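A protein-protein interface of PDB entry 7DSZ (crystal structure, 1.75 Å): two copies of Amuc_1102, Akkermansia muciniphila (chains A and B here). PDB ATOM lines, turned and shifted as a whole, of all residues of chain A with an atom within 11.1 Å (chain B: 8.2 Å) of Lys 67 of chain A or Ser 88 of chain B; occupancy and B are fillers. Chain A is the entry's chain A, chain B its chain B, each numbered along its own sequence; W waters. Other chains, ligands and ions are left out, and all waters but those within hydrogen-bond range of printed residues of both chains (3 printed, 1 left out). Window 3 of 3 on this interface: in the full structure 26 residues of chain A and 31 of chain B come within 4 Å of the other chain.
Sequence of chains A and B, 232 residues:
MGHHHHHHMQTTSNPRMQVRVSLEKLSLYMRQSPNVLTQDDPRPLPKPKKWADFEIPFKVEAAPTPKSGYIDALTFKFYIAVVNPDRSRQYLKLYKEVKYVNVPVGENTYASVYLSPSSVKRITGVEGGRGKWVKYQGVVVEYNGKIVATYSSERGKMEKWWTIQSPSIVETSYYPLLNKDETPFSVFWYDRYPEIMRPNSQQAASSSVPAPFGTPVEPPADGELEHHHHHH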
ATOM      1  N   THR A  11      16.227 -34.307 -15.140  1.00  0.00           N
ATOM      2  CA  THR A  11      17.258 -33.280 -15.164  1.00  0.00           C
ATOM      3  C   THR A  11      18.049 -33.283 -13.861  1.00  0.00           C
ATOM      4  O   THR A  11      17.508 -33.535 -12.780  1.00  0.00           O
ATOM      5  CB  THR A  11      16.647 -31.896 -15.402  1.00  0.00           C
ATOM      6  OG1 THR A  11      17.691 -30.910 -15.433  1.00  0.00           O
ATOM      7  CG2 THR A  11      15.647 -31.538 -14.293  1.00  0.00           C
ATOM      8  N   THR A  12      19.351 -33.032 -13.979  1.00  0.00           N
ATOM      9  CA  THR A  12      20.217 -32.779 -12.834  1.00  0.00           C
ATOM     10  C   THR A  12      20.425 -31.288 -12.600  1.00  0.00           C
ATOM     11  O   THR A  12      21.149 -30.910 -11.674  1.00  0.00           O
ATOM     12  CB  THR A  12      21.573 -33.468 -13.028  1.00  0.00           C
ATOM     13  OG1 THR A  12      22.298 -32.815 -14.074  1.00  0.00           O
ATOM     14  CG2 THR A  12      21.379 -34.925 -13.404  1.00  0.00           C
ATOM     15  N   SER A  13      19.802 -30.444 -13.421  1.00  0.00           N
ATOM     16  CA  SER A  13      19.979 -29.003 -13.403  1.00  0.00           C
ATOM     17  C   SER A  13      18.937 -28.339 -12.509  1.00  0.00           C
ATOM     18  O   SER A  13      18.048 -28.987 -11.949  1.00  0.00           O
ATOM     19  CB  SER A  13      19.873 -28.441 -14.819  1.00  0.00           C
ATOM     20  OG  SER A  13      20.743 -29.108 -15.715  1.00  0.00           O
ATOM     21  N   ASN A  14      19.061 -27.021 -12.371  1.00  0.00           N
ATOM     22  CA  ASN A  14      17.989 -26.196 -11.843  1.00  0.00           C
ATOM     23  C   ASN A  14      16.712 -26.501 -12.623  1.00  0.00           C
ATOM     24  O   ASN A  14      16.696 -26.342 -13.854  1.00  0.00           O
ATOM     25  CB  ASN A  14      18.360 -24.717 -11.961  1.00  0.00           C
ATOM     26  CG  ASN A  14      17.237 -23.773 -11.527  1.00  0.00           C
ATOM     27  OD1 ASN A  14      16.088 -23.896 -11.951  1.00  0.00           O
ATOM     28  ND2 ASN A  14      17.586 -22.808 -10.683  1.00  0.00           N
ATOM     29  N   PRO A  15      15.641 -26.945 -11.960  1.00  0.00           N
ATOM     30  CA  PRO A  15      14.449 -27.390 -12.702  1.00  0.00           C
ATOM     31  C   PRO A  15      13.673 -26.262 -13.366  1.00  0.00           C
ATOM     32  O   PRO A  15      12.808 -26.549 -14.206  1.00  0.00           O
ATOM     33  CB  PRO A  15      13.608 -28.081 -11.625  1.00  0.00           C
ATOM     34  CG  PRO A  15      14.015 -27.400 -10.356  1.00  0.00           C
ATOM     35  CD  PRO A  15      15.477 -27.080 -10.502  1.00  0.00           C
ATOM     36  N   MET A  17      15.099 -24.011 -15.300  1.00  0.00           N
ATOM     37  CA  MET A  17      15.893 -23.529 -16.421  1.00  0.00           C
ATOM     38  C   MET A  17      15.125 -23.657 -17.732  1.00  0.00           C
ATOM     39  O   MET A  17      14.442 -24.652 -17.980  1.00  0.00           O
ATOM     40  CB  MET A  17      17.205 -24.315 -16.491  1.00  0.00           C
ATOM     41  CG  MET A  17      18.227 -23.788 -17.480  1.00  0.00           C
ATOM     42  SD  MET A  17      19.682 -24.863 -17.495  1.00  0.00           S
ATOM     43  CE  MET A  17      18.915 -26.389 -18.035  1.00  0.00           C
ATOM     44  N   ALA A  62      20.665 -20.625 -22.154  1.00  0.00           N
ATOM     45  CA  ALA A  62      19.843 -21.132 -21.069  1.00  0.00           C
ATOM     46  C   ALA A  62      19.655 -20.049 -20.018  1.00  0.00           C
ATOM     47  O   ALA A  62      20.600 -19.331 -19.682  1.00  0.00           O
ATOM     48  CB  ALA A  62      20.463 -22.378 -20.429  1.00  0.00           C
ATOM     49  N   ALA A  63      18.433 -19.951 -19.498  1.00  0.00           N
ATOM     50  CA  ALA A  63      18.073 -18.946 -18.502  1.00  0.00           C
ATOM     51  C   ALA A  63      17.300 -19.624 -17.378  1.00  0.00           C
ATOM     52  O   ALA A  63      16.256 -20.256 -17.640  1.00  0.00           O
ATOM     53  CB  ALA A  63      17.254 -17.819 -19.133  1.00  0.00           C
ATOM     54  N   PRO A  64      17.770 -19.552 -16.124  1.00  0.00           N
ATOM     55  CA  PRO A  64      19.071 -18.970 -15.774  1.00  0.00           C
ATOM     56  C   PRO A  64      20.238 -19.840 -16.261  1.00  0.00           C
ATOM     57  O   PRO A  64      20.071 -21.051 -16.416  1.00  0.00           O
ATOM     58  CB  PRO A  64      19.027 -18.900 -14.241  1.00  0.00           C
ATOM     59  CG  PRO A  64      18.024 -19.911 -13.840  1.00  0.00           C
ATOM     60  CD  PRO A  64      17.003 -19.955 -14.932  1.00  0.00           C
ATOM     61  N   THR A  65      21.372 -19.209 -16.541  1.00  0.00           N
ATOM     62  CA  THR A  65      22.550 -19.944 -16.976  1.00  0.00           C
ATOM     63  C   THR A  65      22.936 -20.964 -15.912  1.00  0.00           C
ATOM     64  O   THR A  65      23.046 -20.607 -14.732  1.00  0.00           O
ATOM     65  CB  THR A  65      23.719 -18.990 -17.226  1.00  0.00           C
ATOM     66  OG1 THR A  65      23.372 -18.052 -18.252  1.00  0.00           O
ATOM     67  CG2 THR A  65      24.959 -19.766 -17.654  1.00  0.00           C
ATOM     68  N   PRO A  66      23.134 -22.230 -16.273  1.00  0.00           N
ATOM     69  CA  PRO A  66      23.543 -23.219 -15.268  1.00  0.00           C
ATOM     70  C   PRO A  66      24.954 -22.960 -14.760  1.00  0.00           C
ATOM     71  O   PRO A  66      25.834 -22.502 -15.494  1.00  0.00           O
ATOM     72  CB  PRO A  66      23.452 -24.554 -16.021  1.00  0.00           C
ATOM     73  CG  PRO A  66      23.453 -24.201 -17.465  1.00  0.00           C
ATOM     74  CD  PRO A  66      22.814 -22.847 -17.572  1.00  0.00           C
ATOM     75  N   LYS A  67      25.153 -23.250 -13.467  1.00  0.00           N
ATOM     76  CA  LYS A  67      26.445 -23.014 -12.825  1.00  0.00           C
ATOM     77  C   LYS A  67      27.566 -23.764 -13.531  1.00  0.00           C
ATOM     78  O   LYS A  67      28.697 -23.270 -13.619  1.00  0.00           O
ATOM     79  CB  LYS A  67      26.392 -23.438 -11.357  1.00  0.00           C
ATOM     80  CG  LYS A  67      25.494 -22.616 -10.463  1.00  0.00           C
ATOM     81  CD  LYS A  67      25.351 -23.293  -9.105  1.00  0.00           C
ATOM     82  CE  LYS A  67      26.703 -23.787  -8.588  1.00  0.00           C
ATOM     83  NZ  LYS A  67      26.578 -24.547  -7.309  1.00  0.00           N
ATOM     84  N   SER A  68      27.274 -24.971 -14.028  1.00  0.00           N
ATOM     85  CA  SER A  68      28.298 -25.810 -14.637  1.00  0.00           C
ATOM     86  C   SER A  68      28.670 -25.370 -16.043  1.00  0.00           C
ATOM     87  O   SER A  68      29.711 -25.800 -16.552  1.00  0.00           O
ATOM     88  CB  SER A  68      27.825 -27.262 -14.677  1.00  0.00           C
ATOM     89  OG  SER A  68      26.709 -27.397 -15.549  1.00  0.00           O
ATOM     90  N   GLY A  69      27.851 -24.534 -16.681  1.00  0.00           N
ATOM     91  CA  GLY A  69      28.109 -24.114 -18.040  1.00  0.00           C
ATOM     92  C   GLY A  69      27.614 -25.070 -19.102  1.00  0.00           C
ATOM     93  O   GLY A  69      27.921 -24.869 -20.281  1.00  0.00           O
ATOM     94  N   TYR A  70      26.851 -26.093 -18.718  1.00  0.00           N
ATOM     95  CA  TYR A  70      26.368 -27.127 -19.618  1.00  0.00           C
ATOM     96  C   TYR A  70      24.928 -27.464 -19.269  1.00  0.00           C
ATOM     97  O   TYR A  70      24.471 -27.236 -18.143  1.00  0.00           O
ATOM     98  CB  TYR A  70      27.190 -28.422 -19.507  1.00  0.00           C
ATOM     99  CG  TYR A  70      28.620 -28.364 -19.970  1.00  0.00           C
ATOM    100  CD1 TYR A  70      29.618 -27.818 -19.164  1.00  0.00           C
ATOM    101  CD2 TYR A  70      28.989 -28.908 -21.197  1.00  0.00           C
ATOM    102  CE1 TYR A  70      30.939 -27.790 -19.582  1.00  0.00           C
ATOM    103  CE2 TYR A  70      30.300 -28.887 -21.618  1.00  0.00           C
ATOM    104  CZ  TYR A  70      31.272 -28.330 -20.807  1.00  0.00           C
ATOM    105  OH  TYR A  70      32.575 -28.314 -21.238  1.00  0.00           O
ATOM    106  N   ILE A  71      24.230 -28.053 -20.238  1.00  0.00           N
ATOM    107  CA  ILE A  71      22.953 -28.705 -19.999  1.00  0.00           C
ATOM    108  C   ILE A  71      23.145 -30.210 -20.190  1.00  0.00           C
ATOM    109  O   ILE A  71      24.107 -30.666 -20.816  1.00  0.00           O
ATOM    110  CB  ILE A  71      21.834 -28.157 -20.910  1.00  0.00           C
ATOM    111  CG1 ILE A  71      22.158 -28.403 -22.380  1.00  0.00           C
ATOM    112  CG2 ILE A  71      21.639 -26.653 -20.685  1.00  0.00           C
ATOM    113  CD1 ILE A  71      20.980 -28.114 -23.288  1.00  0.00           C
ATOM    114  N   ASP A  72      22.215 -30.986 -19.625  1.00  0.00           N
ATOM    115  CA  ASP A  72      22.359 -32.443 -19.583  1.00  0.00           C
ATOM    116  C   ASP A  72      22.469 -33.042 -20.975  1.00  0.00           C
ATOM    117  O   ASP A  72      23.341 -33.883 -21.231  1.00  0.00           O
ATOM    118  CB  ASP A  72      21.169 -33.082 -18.874  1.00  0.00           C
ATOM    119  CG  ASP A  72      21.223 -32.919 -17.376  1.00  0.00           C
ATOM    120  OD1 ASP A  72      22.338 -32.873 -16.822  1.00  0.00           O
ATOM    121  OD2 ASP A  72      20.139 -32.854 -16.769  1.00  0.00           O
ATOM    122  N   VAL A 103      26.051 -30.656 -23.222  1.00  0.00           N
ATOM    123  CA  VAL A 103      26.052 -29.679 -24.307  1.00  0.00           C
ATOM    124  C   VAL A 103      26.416 -28.325 -23.706  1.00  0.00           C
ATOM    125  O   VAL A 103      25.714 -27.862 -22.793  1.00  0.00           O
ATOM    126  CB  VAL A 103      24.704 -29.617 -25.029  1.00  0.00           C
ATOM    127  CG1 VAL A 103      24.793 -28.657 -26.212  1.00  0.00           C
ATOM    128  CG2 VAL A 103      24.276 -31.019 -25.505  1.00  0.00           C
ATOM    129  N   PRO A 104      27.486 -27.683 -24.159  1.00  0.00           N
ATOM    130  CA  PRO A 104      27.900 -26.425 -23.537  1.00  0.00           C
ATOM    131  C   PRO A 104      26.924 -25.313 -23.882  1.00  0.00           C
ATOM    132  O   PRO A 104      26.241 -25.345 -24.908  1.00  0.00           O
ATOM    133  CB  PRO A 104      29.282 -26.171 -24.144  1.00  0.00           C
ATOM    134  CG  PRO A 104      29.211 -26.829 -25.482  1.00  0.00           C
ATOM    135  CD  PRO A 104      28.373 -28.059 -25.275  1.00  0.00           C
ATOM    136  N   VAL A 105      26.834 -24.341 -22.986  1.00  0.00           N
ATOM    137  CA  VAL A 105      25.979 -23.177 -23.172  1.00  0.00           C
ATOM    138  C   VAL A 105      26.840 -22.033 -23.684  1.00  0.00           C
ATOM    139  O   VAL A 105      28.013 -21.906 -23.306  1.00  0.00           O
ATOM    140  CB  VAL A 105      25.261 -22.811 -21.856  1.00  0.00           C
ATOM    141  CG1 VAL A 105      24.534 -21.492 -21.985  1.00  0.00           C
ATOM    142  CG2 VAL A 105      24.285 -23.912 -21.466  1.00  0.00           C
ATOM    143  N   VAL B  82      30.032 -37.669  -7.148  1.00  0.00           N
ATOM    144  CA  VAL B  82      30.627 -36.356  -7.348  1.00  0.00           C
ATOM    145  C   VAL B  82      29.630 -35.312  -6.860  1.00  0.00           C
ATOM    146  O   VAL B  82      28.443 -35.590  -6.677  1.00  0.00           O
ATOM    147  CB  VAL B  82      30.990 -36.082  -8.823  1.00  0.00           C
ATOM    148  CG1 VAL B  82      31.980 -37.119  -9.358  1.00  0.00           C
ATOM    149  CG2 VAL B  82      29.730 -36.052  -9.662  1.00  0.00           C
ATOM    150  N   VAL B  83      30.124 -34.094  -6.670  1.00  0.00           N
ATOM    151  CA  VAL B  83      29.252 -32.974  -6.318  1.00  0.00           C
ATOM    152  C   VAL B  83      28.563 -32.468  -7.580  1.00  0.00           C
ATOM    153  O   VAL B  83      29.226 -32.171  -8.580  1.00  0.00           O
ATOM    154  CB  VAL B  83      30.053 -31.848  -5.641  1.00  0.00           C
ATOM    155  CG1 VAL B  83      29.166 -30.623  -5.431  1.00  0.00           C
ATOM    156  CG2 VAL B  83      30.656 -32.330  -4.323  1.00  0.00           C
ATOM    157  N   ASN B  84      27.231 -32.358  -7.532  1.00  0.00           N
ATOM    158  CA  ASN B  84      26.454 -31.792  -8.633  1.00  0.00           C
ATOM    159  C   ASN B  84      26.887 -30.351  -8.880  1.00  0.00           C
ATOM    160  O   ASN B  84      26.681 -29.484  -8.019  1.00  0.00           O
ATOM    161  CB  ASN B  84      24.952 -31.858  -8.332  1.00  0.00           C
ATOM    162  CG  ASN B  84      24.081 -31.507  -9.542  1.00  0.00           C
ATOM    163  OD1 ASN B  84      24.519 -30.833 -10.477  1.00  0.00           O
ATOM    164  ND2 ASN B  84      22.831 -31.957  -9.515  1.00  0.00           N
ATOM    165  N   PRO B  85      27.474 -30.051 -10.042  1.00  0.00           N
ATOM    166  CA  PRO B  85      27.950 -28.681 -10.296  1.00  0.00           C
ATOM    167  C   PRO B  85      26.835 -27.673 -10.520  1.00  0.00           C
ATOM    168  O   PRO B  85      27.113 -26.466 -10.540  1.00  0.00           O
ATOM    169  CB  PRO B  85      28.807 -28.838 -11.555  1.00  0.00           C
ATOM    170  CG  PRO B  85      28.181 -30.005 -12.273  1.00  0.00           C
ATOM    171  CD  PRO B  85      27.703 -30.944 -11.194  1.00  0.00           C
ATOM    172  N   ASP B  86      25.593 -28.126 -10.694  1.00  0.00           N
ATOM    173  CA  ASP B  86      24.462 -27.236 -10.915  1.00  0.00           C
ATOM    174  C   ASP B  86      23.583 -27.074  -9.683  1.00  0.00           C
ATOM    175  O   ASP B  86      22.738 -26.174  -9.666  1.00  0.00           O
ATOM    176  CB  ASP B  86      23.614 -27.739 -12.093  1.00  0.00           C
ATOM    177  CG  ASP B  86      24.319 -27.574 -13.432  1.00  0.00           C
ATOM    178  OD1 ASP B  86      25.025 -26.560 -13.614  1.00  0.00           O
ATOM    179  OD2 ASP B  86      24.168 -28.458 -14.305  1.00  0.00           O
ATOM    180  N   ARG B  87      23.756 -27.920  -8.662  1.00  0.00           N
ATOM    181  CA  ARG B  87      23.017 -27.812  -7.398  1.00  0.00           C
ATOM    182  C   ARG B  87      23.976 -28.268  -6.299  1.00  0.00           C
ATOM    183  O   ARG B  87      24.128 -29.470  -6.069  1.00  0.00           O
ATOM    184  CB  ARG B  87      21.748 -28.657  -7.421  1.00  0.00           C
ATOM    185  CG  ARG B  87      20.782 -28.320  -8.554  1.00  0.00           C
ATOM    186  CD  ARG B  87      19.774 -29.428  -8.797  1.00  0.00           C
ATOM    187  NE  ARG B  87      18.914 -29.653  -7.640  1.00  0.00           N
ATOM    188  CZ  ARG B  87      17.902 -30.516  -7.619  1.00  0.00           C
ATOM    189  NH1 ARG B  87      17.616 -31.243  -8.696  1.00  0.00           N
ATOM    190  NH2 ARG B  87      17.174 -30.653  -6.519  1.00  0.00           N
ATOM    191  N   SER B  88      24.604 -27.308  -5.616  1.00  0.00           N
ATOM    192  CA  SER B  88      25.819 -27.604  -4.859  1.00  0.00           C
ATOM    193  C   SER B  88      25.586 -28.447  -3.604  1.00  0.00           C
ATOM    194  O   SER B  88      26.542 -29.050  -3.105  1.00  0.00           O
ATOM    195  CB  SER B  88      26.527 -26.307  -4.470  1.00  0.00           C
ATOM    196  OG  SER B  88      27.800 -26.582  -3.910  1.00  0.00           O
ATOM    197  N   ARG B  89      24.361 -28.499  -3.071  1.00  0.00           N
ATOM    198  CA  ARG B  89      24.080 -29.288  -1.876  1.00  0.00           C
ATOM    199  C   ARG B  89      23.691 -30.729  -2.200  1.00  0.00           C
ATOM    200  O   ARG B  89      23.102 -31.411  -1.351  1.00  0.00           O
ATOM    201  CB  ARG B  89      22.981 -28.619  -1.047  1.00  0.00           C
ATOM    202  CG  ARG B  89      23.236 -28.626   0.454  1.00  0.00           C
ATOM    203  CD  ARG B  89      22.721 -27.339   1.083  1.00  0.00           C
ATOM    204  NE  ARG B  89      23.180 -27.130   2.457  1.00  0.00           N
ATOM    205  CZ  ARG B  89      24.427 -26.813   2.797  1.00  0.00           C
ATOM    206  NH1 ARG B  89      25.370 -26.694   1.868  1.00  0.00           N
ATOM    207  NH2 ARG B  89      24.738 -26.625   4.074  1.00  0.00           N
ATOM    208  N   GLN B  90      24.009 -31.205  -3.399  1.00  0.00           N
ATOM    209  CA  GLN B  90      23.557 -32.506  -3.864  1.00  0.00           C
ATOM    210  C   GLN B  90      24.728 -33.277  -4.457  1.00  0.00           C
ATOM    211  O   GLN B  90      25.605 -32.694  -5.104  1.00  0.00           O
ATOM    212  CB  GLN B  90      22.447 -32.357  -4.907  1.00  0.00           C
ATOM    213  CG  GLN B  90      21.703 -33.644  -5.224  1.00  0.00           C
ATOM    214  CD  GLN B  90      20.774 -33.485  -6.407  1.00  0.00           C
ATOM    215  OE1 GLN B  90      21.225 -33.340  -7.544  1.00  0.00           O
ATOM    216  NE2 GLN B  90      19.469 -33.493  -6.146  1.00  0.00           N
ATOM    217  N   TYR B  91      24.745 -34.582  -4.207  1.00  0.00           N
ATOM    218  CA  TYR B  91      25.692 -35.494  -4.831  1.00  0.00           C
ATOM    219  C   TYR B  91      25.021 -36.206  -6.000  1.00  0.00           C
ATOM    220  O   TYR B  91      23.826 -36.528  -5.946  1.00  0.00           O
ATOM    221  CB  TYR B  91      26.215 -36.534  -3.837  1.00  0.00           C
ATOM    222  CG  TYR B  91      27.180 -35.994  -2.810  1.00  0.00           C
ATOM    223  CD1 TYR B  91      28.509 -35.780  -3.127  1.00  0.00           C
ATOM    224  CD2 TYR B  91      26.761 -35.708  -1.512  1.00  0.00           C
ATOM    225  CE1 TYR B  91      29.405 -35.285  -2.186  1.00  0.00           C
ATOM    226  CE2 TYR B  91      27.649 -35.215  -0.564  1.00  0.00           C
ATOM    227  CZ  TYR B  91      28.969 -35.008  -0.910  1.00  0.00           C
ATOM    228  OH  TYR B  91      29.862 -34.521   0.012  1.00  0.00           O
ATOM    229  N   LYS B 121      34.953 -31.627 -17.274  1.00  0.00           N
ATOM    230  CA  LYS B 121      34.933 -30.162 -17.283  1.00  0.00           C
ATOM    231  C   LYS B 121      33.641 -29.624 -16.685  1.00  0.00           C
ATOM    232  O   LYS B 121      33.656 -28.624 -15.951  1.00  0.00           O
ATOM    233  CB  LYS B 121      35.124 -29.628 -18.701  1.00  0.00           C
ATOM    234  CG  LYS B 121      35.050 -28.089 -18.801  1.00  0.00           C
ATOM    235  CD  LYS B 121      35.885 -27.592 -19.982  1.00  0.00           C
ATOM    236  CE  LYS B 121      35.770 -26.076 -20.183  1.00  0.00           C
ATOM    237  NZ  LYS B 121      34.566 -25.721 -20.993  1.00  0.00           N
ATOM    238  N   ARG B 122      32.513 -30.269 -16.982  1.00  0.00           N
ATOM    239  CA  ARG B 122      31.251 -29.840 -16.398  1.00  0.00           C
ATOM    240  C   ARG B 122      31.267 -30.010 -14.883  1.00  0.00           C
ATOM    241  O   ARG B 122      30.834 -29.117 -14.145  1.00  0.00           O
ATOM    242  CB  ARG B 122      30.094 -30.616 -17.020  1.00  0.00           C
ATOM    243  CG  ARG B 122      28.736 -30.182 -16.526  1.00  0.00           C
ATOM    244  CD  ARG B 122      27.613 -30.928 -17.217  1.00  0.00           C
ATOM    245  NE  ARG B 122      26.321 -30.424 -16.772  1.00  0.00           N
ATOM    246  CZ  ARG B 122      25.177 -31.088 -16.863  1.00  0.00           C
ATOM    247  NH1 ARG B 122      25.148 -32.308 -17.405  1.00  0.00           N
ATOM    248  NH2 ARG B 122      24.062 -30.531 -16.405  1.00  0.00           N
ATOM    249  N   ILE B 123      31.790 -31.140 -14.399  1.00  0.00           N
ATOM    250  CA  ILE B 123      31.766 -31.406 -12.961  1.00  0.00           C
ATOM    251  C   ILE B 123      32.651 -30.420 -12.215  1.00  0.00           C
ATOM    252  O   ILE B 123      32.275 -29.914 -11.150  1.00  0.00           O
ATOM    253  CB  ILE B 123      32.205 -32.853 -12.673  1.00  0.00           C
ATOM    254  CG1 ILE B 123      31.128 -33.846 -13.108  1.00  0.00           C
ATOM    255  CG2 ILE B 123      32.542 -33.041 -11.185  1.00  0.00           C
ATOM    256  CD1 ILE B 123      31.675 -35.245 -13.223  1.00  0.00           C
ATOM    257  N   THR B 124      33.841 -30.143 -12.755  1.00  0.00           N
ATOM    258  CA  THR B 124      34.884 -29.450 -12.014  1.00  0.00           C
ATOM    259  C   THR B 124      35.045 -27.989 -12.398  1.00  0.00           C
ATOM    260  O   THR B 124      35.625 -27.226 -11.616  1.00  0.00           O
ATOM    261  CB  THR B 124      36.231 -30.145 -12.216  1.00  0.00           C
ATOM    262  OG1 THR B 124      36.672 -29.949 -13.566  1.00  0.00           O
ATOM    263  CG2 THR B 124      36.107 -31.635 -11.934  1.00  0.00           C
ATOM    264  N   GLY B 125      34.578 -27.592 -13.584  1.00  0.00           N
ATOM    265  CA  GLY B 125      34.741 -26.241 -14.075  1.00  0.00           C
ATOM    266  C   GLY B 125      35.961 -25.994 -14.942  1.00  0.00           C
ATOM    267  O   GLY B 125      36.059 -24.919 -15.544  1.00  0.00           O
ATOM    268  N   SER B 168      20.141 -36.265  -0.432  1.00  0.00           N
ATOM    269  CA  SER B 168      21.316 -35.494  -0.808  1.00  0.00           C
ATOM    270  C   SER B 168      22.155 -36.166  -1.892  1.00  0.00           C
ATOM    271  O   SER B 168      23.158 -35.587  -2.323  1.00  0.00           O
ATOM    272  CB  SER B 168      22.182 -35.239   0.425  1.00  0.00           C
ATOM    273  OG  SER B 168      22.478 -36.461   1.082  1.00  0.00           O
HETATM  274  O   HOH W   1      32.199 -26.378 -16.534  1.00  0.00           O
HETATM  275  O   HOH W   2      24.327 -31.305 -13.226  1.00  0.00           O
HETATM  276  O   HOH W   3      22.622 -24.320 -12.095  1.00  0.00           O
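NH1 of Arg 122 of chain B is in salt-bridge range of OD1 of Asp 72 of chain A, 2.9 Å away.
OG of Ser 68 of chain A is in hydrogen-bond range of NE of Arg 122 of chain B.
The side-chain hydroxyl (OG) of Ser 68 of chain A lies within hydrogen-bond range of the side-chain carboxylate (OD1) of Asp 86 of chain B (2.7 Å).
OH of Tyr 70 of chain A lies within hydrogen-bond range of NZ of Lys 121 of chain B (3.3 Å).
O of Thr 12 of chain A sits at hydrogen-bond distance from ND2 of Asn 84 of chain B (2.9 Å).
The backbone NH (N) of Lys 67 of chain A is in hydrogen-bond range of the side-chain carboxylate (OD1) of Asp 86 of chain B, 3.3 Å away.
The side-chain amide nitrogen (ND2) of Asn 84 of chain B lies within hydrogen-bond range of the side-chain amide oxygen (OE1) of Gln 90 of chain B (2.9 Å).
The backbone NH (N) of Ile 71 of chain A is in hydrogen-bond range of the backbone carbonyl oxygen (O) of Val 103 of chain A (3.0 Å).
The side-chain carboxylate (OD1) of Asp 72 of chain A lies within hydrogen-bond range of the side-chain hydroxyl (OG1) of Thr 12 of chain A, 2.7 Å away.
The backbone NH of Tyr 70 of chain A sits close to the side-chain hydroxyl of Ser 68 of chain A, at 3.4 Å.
OD1 of Asn 84 of chain B sits at hydrogen-bond distance from N of Asp 86 of chain B (2.9 Å).
The guanidinium group of Arg 122 of chain B is in salt-bridge range of the side-chain carboxylate of Asp 86 of chain B.
Among the printed residues, pairs that only touch across the chains: Thr 12 of chain A with Arg 87 of chain B (3.5 Å), Thr 12 of chain A with Arg 122 of chain B (3.7 Å), Ser 13 of chain A with Asp 86 of chain B (3.8 Å), Ser 13 of chain A with Arg 87 of chain B (3.6 Å), Ser 13 of chain A with Arg 122 of chain B (3.7 Å), Pro 66 of chain A with Asp 86 of chain B (3.5 Å), Lys 67 of chain A with Pro 85 of chain B (3.2 Å), Lys 67 of chain A with Ser 88 of chain B (3.3 Å), Ser 68 of chain A with Pro 85 of chain B (3.6 Å), Tyr 70 of chain A with Arg 122 of chain B (3.4 Å) and Ile 71 of chain A with Arg 122 of chain B (3.9 Å).
Of chain B, only Pro 85, Asp 86 and Ser 88 come within 4 Å of Lys 67 of chain A.
Ser 88 of chain B touches just one residue of chain A: Lys 67 (3.3 Å).
Printed residues of chain A within 4 Å of Asn 84 of chain B: Thr 12.
Asp 86 of chain B touches just these residues of chain A: Ser 13, Pro 66, Lys 67 and Ser 68.
Printed residues of chain B within 4 Å of Tyr 70 of chain A: Lys 121 (3.3 Å) and Arg 122 (3.4 Å).
Of the printed residues of chain B, Ser 13 of chain A touches Asp 86 (3.8 Å), Arg 87 (3.6 Å) and Arg 122 (3.7 Å).
The nearest residue of chain A that does not touch Ser 88 of chain B is Thr 12 of chain A (7.8 Å).
The nearest printed residue of chain A that does not touch Lys 121 of chain B is Ser 68 of chain A (4.9 Å).
Of the 20 printed residues of chain A, 8 touch a printed residue of chain B.
Printed residues of chain A that touch a printed residue of chain B: Thr 12, Ser 13, Pro 66, Lys 67, Ser 68, Tyr 70, Ile 71 and Asp 72.
Hydrophobic or aromatic side chains of chain A that line the printed part of chain B: Pro 66 and Tyr 70.
Among the printed residues, Asp or Glu carboxylates within 4 Å of a Lys or Arg side-chain nitrogen of the other chain: Asp 72 of chain A with Arg 122 of chain B (2.9 Å).
No position is printed for both chains.
Of the 17 pairs that touch across the chains among the printed residues, none has its exchanged pair printed and touching as well.
Water W1 lies within hydrogen-bond range of O of Ser 68 of chain A (2.6 Å) and O of Lys 121 of chain B (2.7 Å).
Water W2 lies within hydrogen-bond range of OG1 of Thr 12 of chain A, OD1 of Asn 84 of chain B, OD2 of Asp 86 of chain B and NH2 of Arg 122 of chain B.
Water W3 lies within hydrogen-bond range of O of Asp 86 of chain B and N of Lys 67 of chain A.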
